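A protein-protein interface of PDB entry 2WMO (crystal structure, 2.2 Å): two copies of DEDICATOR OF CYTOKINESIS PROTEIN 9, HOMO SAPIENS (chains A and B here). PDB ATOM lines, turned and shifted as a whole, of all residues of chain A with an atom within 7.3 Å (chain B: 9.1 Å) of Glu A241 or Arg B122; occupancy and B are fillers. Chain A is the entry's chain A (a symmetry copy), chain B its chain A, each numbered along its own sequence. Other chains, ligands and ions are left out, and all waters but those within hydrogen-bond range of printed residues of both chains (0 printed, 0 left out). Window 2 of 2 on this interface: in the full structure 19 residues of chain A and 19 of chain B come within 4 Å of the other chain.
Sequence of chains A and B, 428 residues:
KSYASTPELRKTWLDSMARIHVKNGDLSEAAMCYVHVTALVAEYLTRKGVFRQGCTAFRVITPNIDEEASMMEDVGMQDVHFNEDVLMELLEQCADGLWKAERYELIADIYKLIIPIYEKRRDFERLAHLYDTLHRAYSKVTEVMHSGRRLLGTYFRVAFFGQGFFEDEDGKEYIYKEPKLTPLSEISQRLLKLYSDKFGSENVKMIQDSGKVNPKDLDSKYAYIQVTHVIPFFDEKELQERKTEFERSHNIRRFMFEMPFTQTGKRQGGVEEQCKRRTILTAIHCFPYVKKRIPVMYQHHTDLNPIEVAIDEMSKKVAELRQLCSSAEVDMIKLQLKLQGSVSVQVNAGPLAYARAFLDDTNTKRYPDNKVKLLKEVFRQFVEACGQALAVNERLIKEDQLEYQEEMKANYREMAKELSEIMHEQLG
The guanidinium group (NH1) of Arg B122 sits at hydrogen-bond distance from the backbone carbonyl oxygen (O) of Glu A241 (3.3 Å). OE2 of Glu A247 lies within salt-bridge range of NE of Arg B122, 2.5 Å away.
The backbone carbonyl oxygen of Lys B120 is in hydrogen-bond range of the guanidinium group of Arg B122 (3.0 Å). OE2 of Glu A241 lies within salt-bridge range of NZ of Lys A237, 3.2 Å away. The backbone carbonyl oxygen of Gln A240 lies close to the side-chain amino group of Lys A243 (3.4 Å). O of Glu A247 is in hydrogen-bond range of NH1 of Arg A242, at 2.9 Å. N of Lys A243 lies within hydrogen-bond range of OE1 of Glu A247 (2.8 Å). OG1 of Thr A244 is in hydrogen-bond range of N of Glu A247.
Val A141 touches Phe B124 (CG1 to CG, 3.7 Å). CB of Phe B124 touches CG2 of Thr A142 (3.7 Å). Glu B125 touches Thr A142. Met A145 touches Phe B124. NH1 of Arg B122 touches CG of Lys A243, 2.9 Å away.
Glu A241 touches just one residue of chain B: Arg B122 (3.3 Å). Of chain A, only Glu A241 (3.3 Å), Lys A243 (2.9 Å) and Glu A247 (2.5 Å) come within 4 Å of Arg B122. Printed residues of chain B within 4 Å of Val A141: Phe B124 (3.7 Å). Of the printed residues of chain A, Phe B124 touches Val A141, Thr A142 and Met A145. The nearest residue of chain A that does not touch Arg B122 is Thr A244 (4.6 Å).
Along chain A the printed residues that touch a printed residue of chain B span positions 141 to 247. Printed residues of chain B that touch a printed residue of chain A: Arg B122, Phe B124 and Glu B125. Hydrophobic or aromatic side chains of chain B within 4 Å of the printed part of chain A: Phe B124. Among the printed residues, 7 pairs touch across the chains.
No position is printed for both chains. Of the 7 pairs that touch across the chains among the printed residues, none has its exchanged pair printed and touching as well.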
ATOM      1  N   VAL A 141     -41.352 -24.178 -28.611  1.00  0.00           N
ATOM      2  CA  VAL A 141     -40.098 -24.653 -28.006  1.00  0.00           C
ATOM      3  C   VAL A 141     -39.400 -23.580 -27.170  1.00  0.00           C
ATOM      4  O   VAL A 141     -38.979 -23.834 -26.046  1.00  0.00           O
ATOM      5  CB  VAL A 141     -39.106 -25.273 -29.049  1.00  0.00           C
ATOM      6  CG1 VAL A 141     -37.743 -25.537 -28.414  1.00  0.00           C
ATOM      7  CG2 VAL A 141     -39.667 -26.571 -29.601  1.00  0.00           C
ATOM      8  N   THR A 142     -39.275 -22.368 -27.700  1.00  0.00           N
ATOM      9  CA  THR A 142     -38.590 -21.333 -26.931  1.00  0.00           C
ATOM     10  C   THR A 142     -39.449 -20.858 -25.763  1.00  0.00           C
ATOM     11  O   THR A 142     -38.931 -20.433 -24.738  1.00  0.00           O
ATOM     12  CB  THR A 142     -38.171 -20.113 -27.794  1.00  0.00           C
ATOM     13  OG1 THR A 142     -39.340 -19.505 -28.346  1.00  0.00           O
ATOM     14  CG2 THR A 142     -37.225 -20.530 -28.920  1.00  0.00           C
ATOM     15  N   MET A 145     -39.184 -23.631 -23.024  1.00  0.00           N
ATOM     16  CA  MET A 145     -37.818 -23.676 -22.535  1.00  0.00           C
ATOM     17  C   MET A 145     -37.583 -22.584 -21.495  1.00  0.00           C
ATOM     18  O   MET A 145     -36.724 -22.727 -20.620  1.00  0.00           O
ATOM     19  CB  MET A 145     -36.808 -23.551 -23.673  1.00  0.00           C
ATOM     20  CG  MET A 145     -36.671 -24.802 -24.517  1.00  0.00           C
ATOM     21  SD  MET A 145     -35.412 -24.606 -25.804  1.00  0.00           S
ATOM     22  CE  MET A 145     -33.910 -24.387 -24.840  1.00  0.00           C
ATOM     23  N   ASP A 235     -24.696 -40.381 -18.112  1.00  0.00           N
ATOM     24  CA  ASP A 235     -23.278 -40.235 -17.792  1.00  0.00           C
ATOM     25  C   ASP A 235     -22.791 -38.899 -18.340  1.00  0.00           C
ATOM     26  O   ASP A 235     -23.540 -38.208 -19.040  1.00  0.00           O
ATOM     27  CB  ASP A 235     -22.459 -41.401 -18.363  1.00  0.00           C
ATOM     28  CG  ASP A 235     -22.491 -41.456 -19.879  1.00  0.00           C
ATOM     29  OD1 ASP A 235     -22.286 -40.402 -20.529  1.00  0.00           O
ATOM     30  OD2 ASP A 235     -22.702 -42.563 -20.421  1.00  0.00           O
ATOM     31  N   GLU A 236     -21.545 -38.538 -18.030  1.00  0.00           N
ATOM     32  CA  GLU A 236     -21.007 -37.221 -18.385  1.00  0.00           C
ATOM     33  C   GLU A 236     -21.033 -36.954 -19.890  1.00  0.00           C
ATOM     34  O   GLU A 236     -21.338 -35.847 -20.341  1.00  0.00           O
ATOM     35  CB  GLU A 236     -19.577 -37.062 -17.858  1.00  0.00           C
ATOM     36  N   LYS A 237     -20.696 -37.975 -20.657  1.00  0.00           N
ATOM     37  CA  LYS A 237     -20.721 -37.891 -22.099  1.00  0.00           C
ATOM     38  C   LYS A 237     -22.154 -37.654 -22.592  1.00  0.00           C
ATOM     39  O   LYS A 237     -22.394 -36.786 -23.432  1.00  0.00           O
ATOM     40  CB  LYS A 237     -20.146 -39.180 -22.684  1.00  0.00           C
ATOM     41  CG  LYS A 237     -20.139 -39.243 -24.190  1.00  0.00           C
ATOM     42  CD  LYS A 237     -19.967 -40.688 -24.641  1.00  0.00           C
ATOM     43  CE  LYS A 237     -20.077 -40.803 -26.151  1.00  0.00           C
ATOM     44  NZ  LYS A 237     -19.285 -39.730 -26.821  1.00  0.00           N
ATOM     45  N   GLU A 238     -23.101 -38.426 -22.067  1.00  0.00           N
ATOM     46  CA  GLU A 238     -24.500 -38.239 -22.412  1.00  0.00           C
ATOM     47  C   GLU A 238     -24.980 -36.846 -22.035  1.00  0.00           C
ATOM     48  O   GLU A 238     -25.757 -36.243 -22.761  1.00  0.00           O
ATOM     49  CB  GLU A 238     -25.370 -39.301 -21.738  1.00  0.00           C
ATOM     50  CG  GLU A 238     -25.348 -40.647 -22.429  1.00  0.00           C
ATOM     51  CD  GLU A 238     -26.131 -41.685 -21.664  1.00  0.00           C
ATOM     52  OE1 GLU A 238     -26.027 -41.693 -20.423  1.00  0.00           O
ATOM     53  OE2 GLU A 238     -26.855 -42.479 -22.301  1.00  0.00           O
ATOM     54  N   LEU A 239     -24.518 -36.334 -20.899  1.00  0.00           N
ATOM     55  CA  LEU A 239     -24.894 -34.993 -20.461  1.00  0.00           C
ATOM     56  C   LEU A 239     -24.302 -33.923 -21.375  1.00  0.00           C
ATOM     57  O   LEU A 239     -24.806 -32.803 -21.451  1.00  0.00           O
ATOM     58  CB  LEU A 239     -24.449 -34.742 -19.024  1.00  0.00           C
ATOM     59  CG  LEU A 239     -25.103 -35.648 -17.976  1.00  0.00           C
ATOM     60  CD1 LEU A 239     -24.173 -35.882 -16.795  1.00  0.00           C
ATOM     61  CD2 LEU A 239     -26.438 -35.081 -17.513  1.00  0.00           C
ATOM     62  N   GLN A 240     -23.227 -34.275 -22.064  1.00  0.00           N
ATOM     63  CA  GLN A 240     -22.603 -33.344 -22.982  1.00  0.00           C
ATOM     64  C   GLN A 240     -23.378 -33.399 -24.285  1.00  0.00           C
ATOM     65  O   GLN A 240     -23.603 -32.366 -24.918  1.00  0.00           O
ATOM     66  CB  GLN A 240     -21.129 -33.693 -23.202  1.00  0.00           C
ATOM     67  N   GLU A 241     -23.803 -34.600 -24.675  1.00  0.00           N
ATOM     68  CA  GLU A 241     -24.550 -34.774 -25.926  1.00  0.00           C
ATOM     69  C   GLU A 241     -25.985 -34.277 -25.801  1.00  0.00           C
ATOM     70  O   GLU A 241     -26.551 -33.754 -26.750  1.00  0.00           O
ATOM     71  CB  GLU A 241     -24.566 -36.237 -26.370  1.00  0.00           C
ATOM     72  CG  GLU A 241     -23.200 -36.899 -26.421  1.00  0.00           C
ATOM     73  CD  GLU A 241     -23.275 -38.414 -26.561  1.00  0.00           C
ATOM     74  OE1 GLU A 241     -24.223 -39.033 -26.024  1.00  0.00           O
ATOM     75  OE2 GLU A 241     -22.370 -38.991 -27.199  1.00  0.00           O
ATOM     76  N   ARG A 242     -26.583 -34.472 -24.635  1.00  0.00           N
ATOM     77  CA  ARG A 242     -27.960 -34.054 -24.426  1.00  0.00           C
ATOM     78  C   ARG A 242     -27.946 -32.679 -23.768  1.00  0.00           C
ATOM     79  O   ARG A 242     -27.860 -32.558 -22.547  1.00  0.00           O
ATOM     80  CB  ARG A 242     -28.711 -35.092 -23.584  1.00  0.00           C
ATOM     81  CG  ARG A 242     -28.895 -36.429 -24.314  1.00  0.00           C
ATOM     82  CD  ARG A 242     -29.221 -37.559 -23.371  1.00  0.00           C
ATOM     83  NE  ARG A 242     -29.320 -38.856 -24.040  1.00  0.00           N
ATOM     84  CZ  ARG A 242     -30.456 -39.409 -24.454  1.00  0.00           C
ATOM     85  NH1 ARG A 242     -31.608 -38.772 -24.301  1.00  0.00           N
ATOM     86  NH2 ARG A 242     -30.443 -40.599 -25.045  1.00  0.00           N
ATOM     87  N   LYS A 243     -28.008 -31.630 -24.580  1.00  0.00           N
ATOM     88  CA  LYS A 243     -27.722 -30.302 -24.048  1.00  0.00           C
ATOM     89  C   LYS A 243     -28.920 -29.592 -23.420  1.00  0.00           C
ATOM     90  O   LYS A 243     -28.751 -28.763 -22.521  1.00  0.00           O
ATOM     91  CB  LYS A 243     -27.006 -29.428 -25.092  1.00  0.00           C
ATOM     92  CG  LYS A 243     -27.184 -29.881 -26.546  1.00  0.00           C
ATOM     93  CD  LYS A 243     -25.921 -29.611 -27.375  1.00  0.00           C
ATOM     94  CE  LYS A 243     -24.956 -30.807 -27.309  1.00  0.00           C
ATOM     95  NZ  LYS A 243     -23.575 -30.494 -27.805  1.00  0.00           N
ATOM     96  N   THR A 244     -30.125 -29.931 -23.867  1.00  0.00           N
ATOM     97  CA  THR A 244     -31.321 -29.270 -23.370  1.00  0.00           C
ATOM     98  C   THR A 244     -32.140 -30.173 -22.442  1.00  0.00           C
ATOM     99  O   THR A 244     -31.921 -31.386 -22.368  1.00  0.00           O
ATOM    100  CB  THR A 244     -32.225 -28.817 -24.518  1.00  0.00           C
ATOM    101  OG1 THR A 244     -32.773 -29.967 -25.161  1.00  0.00           O
ATOM    102  CG2 THR A 244     -31.437 -27.982 -25.556  1.00  0.00           C
ATOM    103  N   GLU A 247     -33.861 -32.782 -24.612  1.00  0.00           N
ATOM    104  CA  GLU A 247     -33.017 -33.896 -25.058  1.00  0.00           C
ATOM    105  C   GLU A 247     -32.745 -34.878 -23.906  1.00  0.00           C
ATOM    106  O   GLU A 247     -32.319 -36.010 -24.131  1.00  0.00           O
ATOM    107  CB  GLU A 247     -31.706 -33.406 -25.680  1.00  0.00           C
ATOM    108  CG  GLU A 247     -31.896 -32.556 -26.956  1.00  0.00           C
ATOM    109  CD  GLU A 247     -30.607 -31.892 -27.433  1.00  0.00           C
ATOM    110  OE1 GLU A 247     -29.540 -32.152 -26.842  1.00  0.00           O
ATOM    111  OE2 GLU A 247     -30.670 -31.095 -28.393  1.00  0.00           O
ATOM    112  N   ARG A 248     -33.004 -34.432 -22.682  1.00  0.00           N
ATOM    113  CA  ARG A 248     -32.829 -35.267 -21.496  1.00  0.00           C
ATOM    114  C   ARG A 248     -34.156 -35.892 -21.052  1.00  0.00           C
ATOM    115  O   ARG A 248     -34.245 -36.495 -19.973  1.00  0.00           O
ATOM    116  CB  ARG A 248     -32.218 -34.446 -20.359  1.00  0.00           C
ATOM    117  CG  ARG A 248     -30.755 -34.142 -20.584  1.00  0.00           C
ATOM    118  CD  ARG A 248     -30.194 -33.174 -19.571  1.00  0.00           C
ATOM    119  NE  ARG A 248     -28.818 -32.832 -19.924  1.00  0.00           N
ATOM    120  CZ  ARG A 248     -27.958 -32.219 -19.113  1.00  0.00           C
ATOM    121  NH1 ARG A 248     -28.319 -31.871 -17.882  1.00  0.00           N
ATOM    122  NH2 ARG A 248     -26.728 -31.954 -19.533  1.00  0.00           N
ATOM    123  N   ILE B 115     -30.972 -25.014 -42.358  1.00  0.00           N
ATOM    124  CA  ILE B 115     -31.785 -25.668 -41.333  1.00  0.00           C
ATOM    125  C   ILE B 115     -30.968 -26.655 -40.478  1.00  0.00           C
ATOM    126  O   ILE B 115     -31.018 -26.579 -39.270  1.00  0.00           O
ATOM    127  CB  ILE B 115     -33.089 -26.273 -41.929  1.00  0.00           C
ATOM    128  CG1 ILE B 115     -34.143 -25.170 -42.096  1.00  0.00           C
ATOM    129  CG2 ILE B 115     -33.649 -27.448 -41.068  1.00  0.00           C
ATOM    130  CD1 ILE B 115     -35.291 -25.559 -43.027  1.00  0.00           C
ATOM    131  N   PRO B 116     -30.152 -27.526 -41.105  1.00  0.00           N
ATOM    132  CA  PRO B 116     -29.361 -28.452 -40.280  1.00  0.00           C
ATOM    133  C   PRO B 116     -28.330 -27.757 -39.397  1.00  0.00           C
ATOM    134  O   PRO B 116     -27.939 -28.292 -38.350  1.00  0.00           O
ATOM    135  CB  PRO B 116     -28.668 -29.353 -41.320  1.00  0.00           C
ATOM    136  CG  PRO B 116     -29.560 -29.267 -42.550  1.00  0.00           C
ATOM    137  CD  PRO B 116     -30.043 -27.838 -42.544  1.00  0.00           C
ATOM    138  N   ILE B 117     -27.894 -26.569 -39.796  1.00  0.00           N
ATOM    139  CA  ILE B 117     -26.937 -25.839 -38.994  1.00  0.00           C
ATOM    140  C   ILE B 117     -27.625 -25.266 -37.763  1.00  0.00           C
ATOM    141  O   ILE B 117     -27.137 -25.418 -36.655  1.00  0.00           O
ATOM    142  CB  ILE B 117     -26.238 -24.702 -39.797  1.00  0.00           C
ATOM    143  CG1 ILE B 117     -25.402 -25.271 -40.943  1.00  0.00           C
ATOM    144  CG2 ILE B 117     -25.370 -23.865 -38.890  1.00  0.00           C
ATOM    145  CD1 ILE B 117     -24.791 -24.211 -41.821  1.00  0.00           C
ATOM    146  N   TYR B 118     -28.758 -24.604 -37.957  1.00  0.00           N
ATOM    147  CA  TYR B 118     -29.539 -24.129 -36.817  1.00  0.00           C
ATOM    148  C   TYR B 118     -29.938 -25.271 -35.844  1.00  0.00           C
ATOM    149  O   TYR B 118     -29.901 -25.082 -34.638  1.00  0.00           O
ATOM    150  CB  TYR B 118     -30.780 -23.364 -37.272  1.00  0.00           C
ATOM    151  CG  TYR B 118     -30.509 -21.982 -37.852  1.00  0.00           C
ATOM    152  CD1 TYR B 118     -29.463 -21.184 -37.383  1.00  0.00           C
ATOM    153  CD2 TYR B 118     -31.320 -21.470 -38.866  1.00  0.00           C
ATOM    154  CE1 TYR B 118     -29.239 -19.906 -37.920  1.00  0.00           C
ATOM    155  CE2 TYR B 118     -31.113 -20.222 -39.393  1.00  0.00           C
ATOM    156  CZ  TYR B 118     -30.066 -19.441 -38.932  1.00  0.00           C
ATOM    157  OH  TYR B 118     -29.889 -18.182 -39.476  1.00  0.00           O
ATOM    158  N   GLU B 119     -30.296 -26.445 -36.376  1.00  0.00           N
ATOM    159  CA  GLU B 119     -30.661 -27.583 -35.528  1.00  0.00           C
ATOM    160  C   GLU B 119     -29.472 -28.019 -34.685  1.00  0.00           C
ATOM    161  O   GLU B 119     -29.575 -28.141 -33.467  1.00  0.00           O
ATOM    162  CB  GLU B 119     -31.193 -28.750 -36.375  1.00  0.00           C
ATOM    163  CG  GLU B 119     -32.493 -28.400 -37.120  1.00  0.00           C
ATOM    164  CD  GLU B 119     -32.937 -29.478 -38.093  1.00  0.00           C
ATOM    165  OE1 GLU B 119     -32.068 -30.158 -38.658  1.00  0.00           O
ATOM    166  OE2 GLU B 119     -34.161 -29.638 -38.307  1.00  0.00           O
ATOM    167  N   LYS B 120     -28.329 -28.234 -35.329  1.00  0.00           N
ATOM    168  CA  LYS B 120     -27.115 -28.583 -34.591  1.00  0.00           C
ATOM    169  C   LYS B 120     -26.747 -27.528 -33.535  1.00  0.00           C
ATOM    170  O   LYS B 120     -26.232 -27.864 -32.474  1.00  0.00           O
ATOM    171  CB  LYS B 120     -25.955 -28.827 -35.558  1.00  0.00           C
ATOM    172  CG  LYS B 120     -24.581 -28.865 -34.906  1.00  0.00           C
ATOM    173  N   ARG B 121     -27.030 -26.261 -33.816  1.00  0.00           N
ATOM    174  CA  ARG B 121     -26.714 -25.201 -32.871  1.00  0.00           C
ATOM    175  C   ARG B 121     -27.789 -25.007 -31.797  1.00  0.00           C
ATOM    176  O   ARG B 121     -27.630 -24.172 -30.896  1.00  0.00           O
ATOM    177  CB  ARG B 121     -26.438 -23.866 -33.609  1.00  0.00           C
ATOM    178  CG  ARG B 121     -25.065 -23.804 -34.299  1.00  0.00           C
ATOM    179  CD  ARG B 121     -24.739 -22.417 -34.894  1.00  0.00           C
ATOM    180  NE  ARG B 121     -23.507 -22.467 -35.685  1.00  0.00           N
ATOM    181  CZ  ARG B 121     -22.795 -21.398 -36.054  1.00  0.00           C
ATOM    182  NH1 ARG B 121     -23.181 -20.185 -35.704  1.00  0.00           N
ATOM    183  NH2 ARG B 121     -21.686 -21.545 -36.772  1.00  0.00           N
ATOM    184  N   ARG B 122     -28.871 -25.780 -31.896  1.00  0.00           N
ATOM    185  CA  ARG B 122     -30.077 -25.608 -31.070  1.00  0.00           C
ATOM    186  C   ARG B 122     -30.648 -24.194 -31.157  1.00  0.00           C
ATOM    187  O   ARG B 122     -31.197 -23.668 -30.179  1.00  0.00           O
ATOM    188  CB  ARG B 122     -29.830 -25.954 -29.600  1.00  0.00           C
ATOM    189  CG  ARG B 122     -28.913 -27.132 -29.339  1.00  0.00           C
ATOM    190  CD  ARG B 122     -29.370 -28.405 -29.963  1.00  0.00           C
ATOM    191  NE  ARG B 122     -28.861 -29.576 -29.243  1.00  0.00           N
ATOM    192  CZ  ARG B 122     -27.912 -30.403 -29.691  1.00  0.00           C
ATOM    193  NH1 ARG B 122     -27.534 -31.443 -28.953  1.00  0.00           N
ATOM    194  NH2 ARG B 122     -27.327 -30.197 -30.864  1.00  0.00           N
ATOM    195  N   ASP B 123     -30.535 -23.572 -32.325  1.00  0.00           N
ATOM    196  CA  ASP B 123     -31.006 -22.200 -32.445  1.00  0.00           C
ATOM    197  C   ASP B 123     -32.475 -22.211 -32.818  1.00  0.00           C
ATOM    198  O   ASP B 123     -32.841 -22.095 -33.991  1.00  0.00           O
ATOM    199  CB  ASP B 123     -30.167 -21.426 -33.468  1.00  0.00           C
ATOM    200  CG  ASP B 123     -30.300 -19.920 -33.315  1.00  0.00           C
ATOM    201  OD1 ASP B 123     -31.340 -19.455 -32.793  1.00  0.00           O
ATOM    202  OD2 ASP B 123     -29.374 -19.196 -33.742  1.00  0.00           O
ATOM    203  N   PHE B 124     -33.321 -22.360 -31.809  1.00  0.00           N
ATOM    204  CA  PHE B 124     -34.739 -22.547 -32.033  1.00  0.00           C
ATOM    205  C   PHE B 124     -35.454 -21.267 -32.473  1.00  0.00           C
ATOM    206  O   PHE B 124     -36.425 -21.332 -33.208  1.00  0.00           O
ATOM    207  CB  PHE B 124     -35.406 -23.168 -30.784  1.00  0.00           C
ATOM    208  CG  PHE B 124     -34.789 -24.488 -30.359  1.00  0.00           C
ATOM    209  CD1 PHE B 124     -34.807 -25.586 -31.211  1.00  0.00           C
ATOM    210  CD2 PHE B 124     -34.193 -24.627 -29.111  1.00  0.00           C
ATOM    211  CE1 PHE B 124     -34.235 -26.792 -30.831  1.00  0.00           C
ATOM    212  CE2 PHE B 124     -33.605 -25.831 -28.728  1.00  0.00           C
ATOM    213  CZ  PHE B 124     -33.634 -26.912 -29.579  1.00  0.00           C
ATOM    214  N   GLU B 125     -35.000 -20.110 -32.011  1.00  0.00           N
ATOM    215  CA  GLU B 125     -35.599 -18.843 -32.448  1.00  0.00           C
ATOM    216  C   GLU B 125     -35.344 -18.545 -33.940  1.00  0.00           C
ATOM    217  O   GLU B 125     -36.237 -18.077 -34.641  1.00  0.00           O
ATOM    218  CB  GLU B 125     -35.119 -17.667 -31.584  1.00  0.00           C
ATOM    219  CG  GLU B 125     -36.116 -16.487 -31.553  1.00  0.00           C
ATOM    220  CD  GLU B 125     -36.283 -15.804 -32.917  1.00  0.00           C
ATOM    221  OE1 GLU B 125     -35.314 -15.156 -33.387  1.00  0.00           O
ATOM    222  OE2 GLU B 125     -37.388 -15.910 -33.519  1.00  0.00           O
ATOM    223  N   ARG B 126     -34.136 -18.829 -34.415  1.00  0.00           N
ATOM    224  CA  ARG B 126     -33.820 -18.700 -35.843  1.00  0.00           C
ATOM    225  C   ARG B 126     -34.640 -19.684 -36.668  1.00  0.00           C
ATOM    226  O   ARG B 126     -35.095 -19.368 -37.768  1.00  0.00           O
ATOM    227  CB  ARG B 126     -32.344 -18.977 -36.103  1.00  0.00           C
ATOM    228  CG  ARG B 126     -31.371 -18.011 -35.459  1.00  0.00           C
ATOM    229  CD  ARG B 126     -31.518 -16.609 -35.958  1.00  0.00           C
ATOM    230  NE  ARG B 126     -30.221 -15.944 -36.125  1.00  0.00           N
ATOM    231  CZ  ARG B 126     -29.395 -15.624 -35.130  1.00  0.00           C
ATOM    232  NH1 ARG B 126     -29.695 -15.934 -33.871  1.00  0.00           N
ATOM    233  NH2 ARG B 126     -28.245 -15.013 -35.392  1.00  0.00           N
ATOM    234  N   LEU B 127     -34.818 -20.893 -36.138  1.00  0.00           N
ATOM    235  CA  LEU B 127     -35.646 -21.874 -36.814  1.00  0.00           C
ATOM    236  C   LEU B 127     -37.077 -21.349 -36.892  1.00  0.00           C
ATOM    237  O   LEU B 127     -37.707 -21.411 -37.934  1.00  0.00           O
ATOM    238  CB  LEU B 127     -35.575 -23.223 -36.073  1.00  0.00           C
ATOM    239  CG  LEU B 127     -34.254 -23.951 -36.376  1.00  0.00           C
ATOM    240  CD1 LEU B 127     -33.993 -25.072 -35.406  1.00  0.00           C
ATOM    241  CD2 LEU B 127     -34.261 -24.476 -37.828  1.00  0.00           C
ATOM    242  N   ALA B 128     -37.587 -20.837 -35.776  1.00  0.00           N
ATOM    243  CA  ALA B 128     -38.947 -20.299 -35.736  1.00  0.00           C
ATOM    244  C   ALA B 128     -39.152 -19.227 -36.810  1.00  0.00           C
ATOM    245  O   ALA B 128     -40.184 -19.179 -37.465  1.00  0.00           O
ATOM    246  CB  ALA B 128     -39.240 -19.713 -34.342  1.00  0.00           C
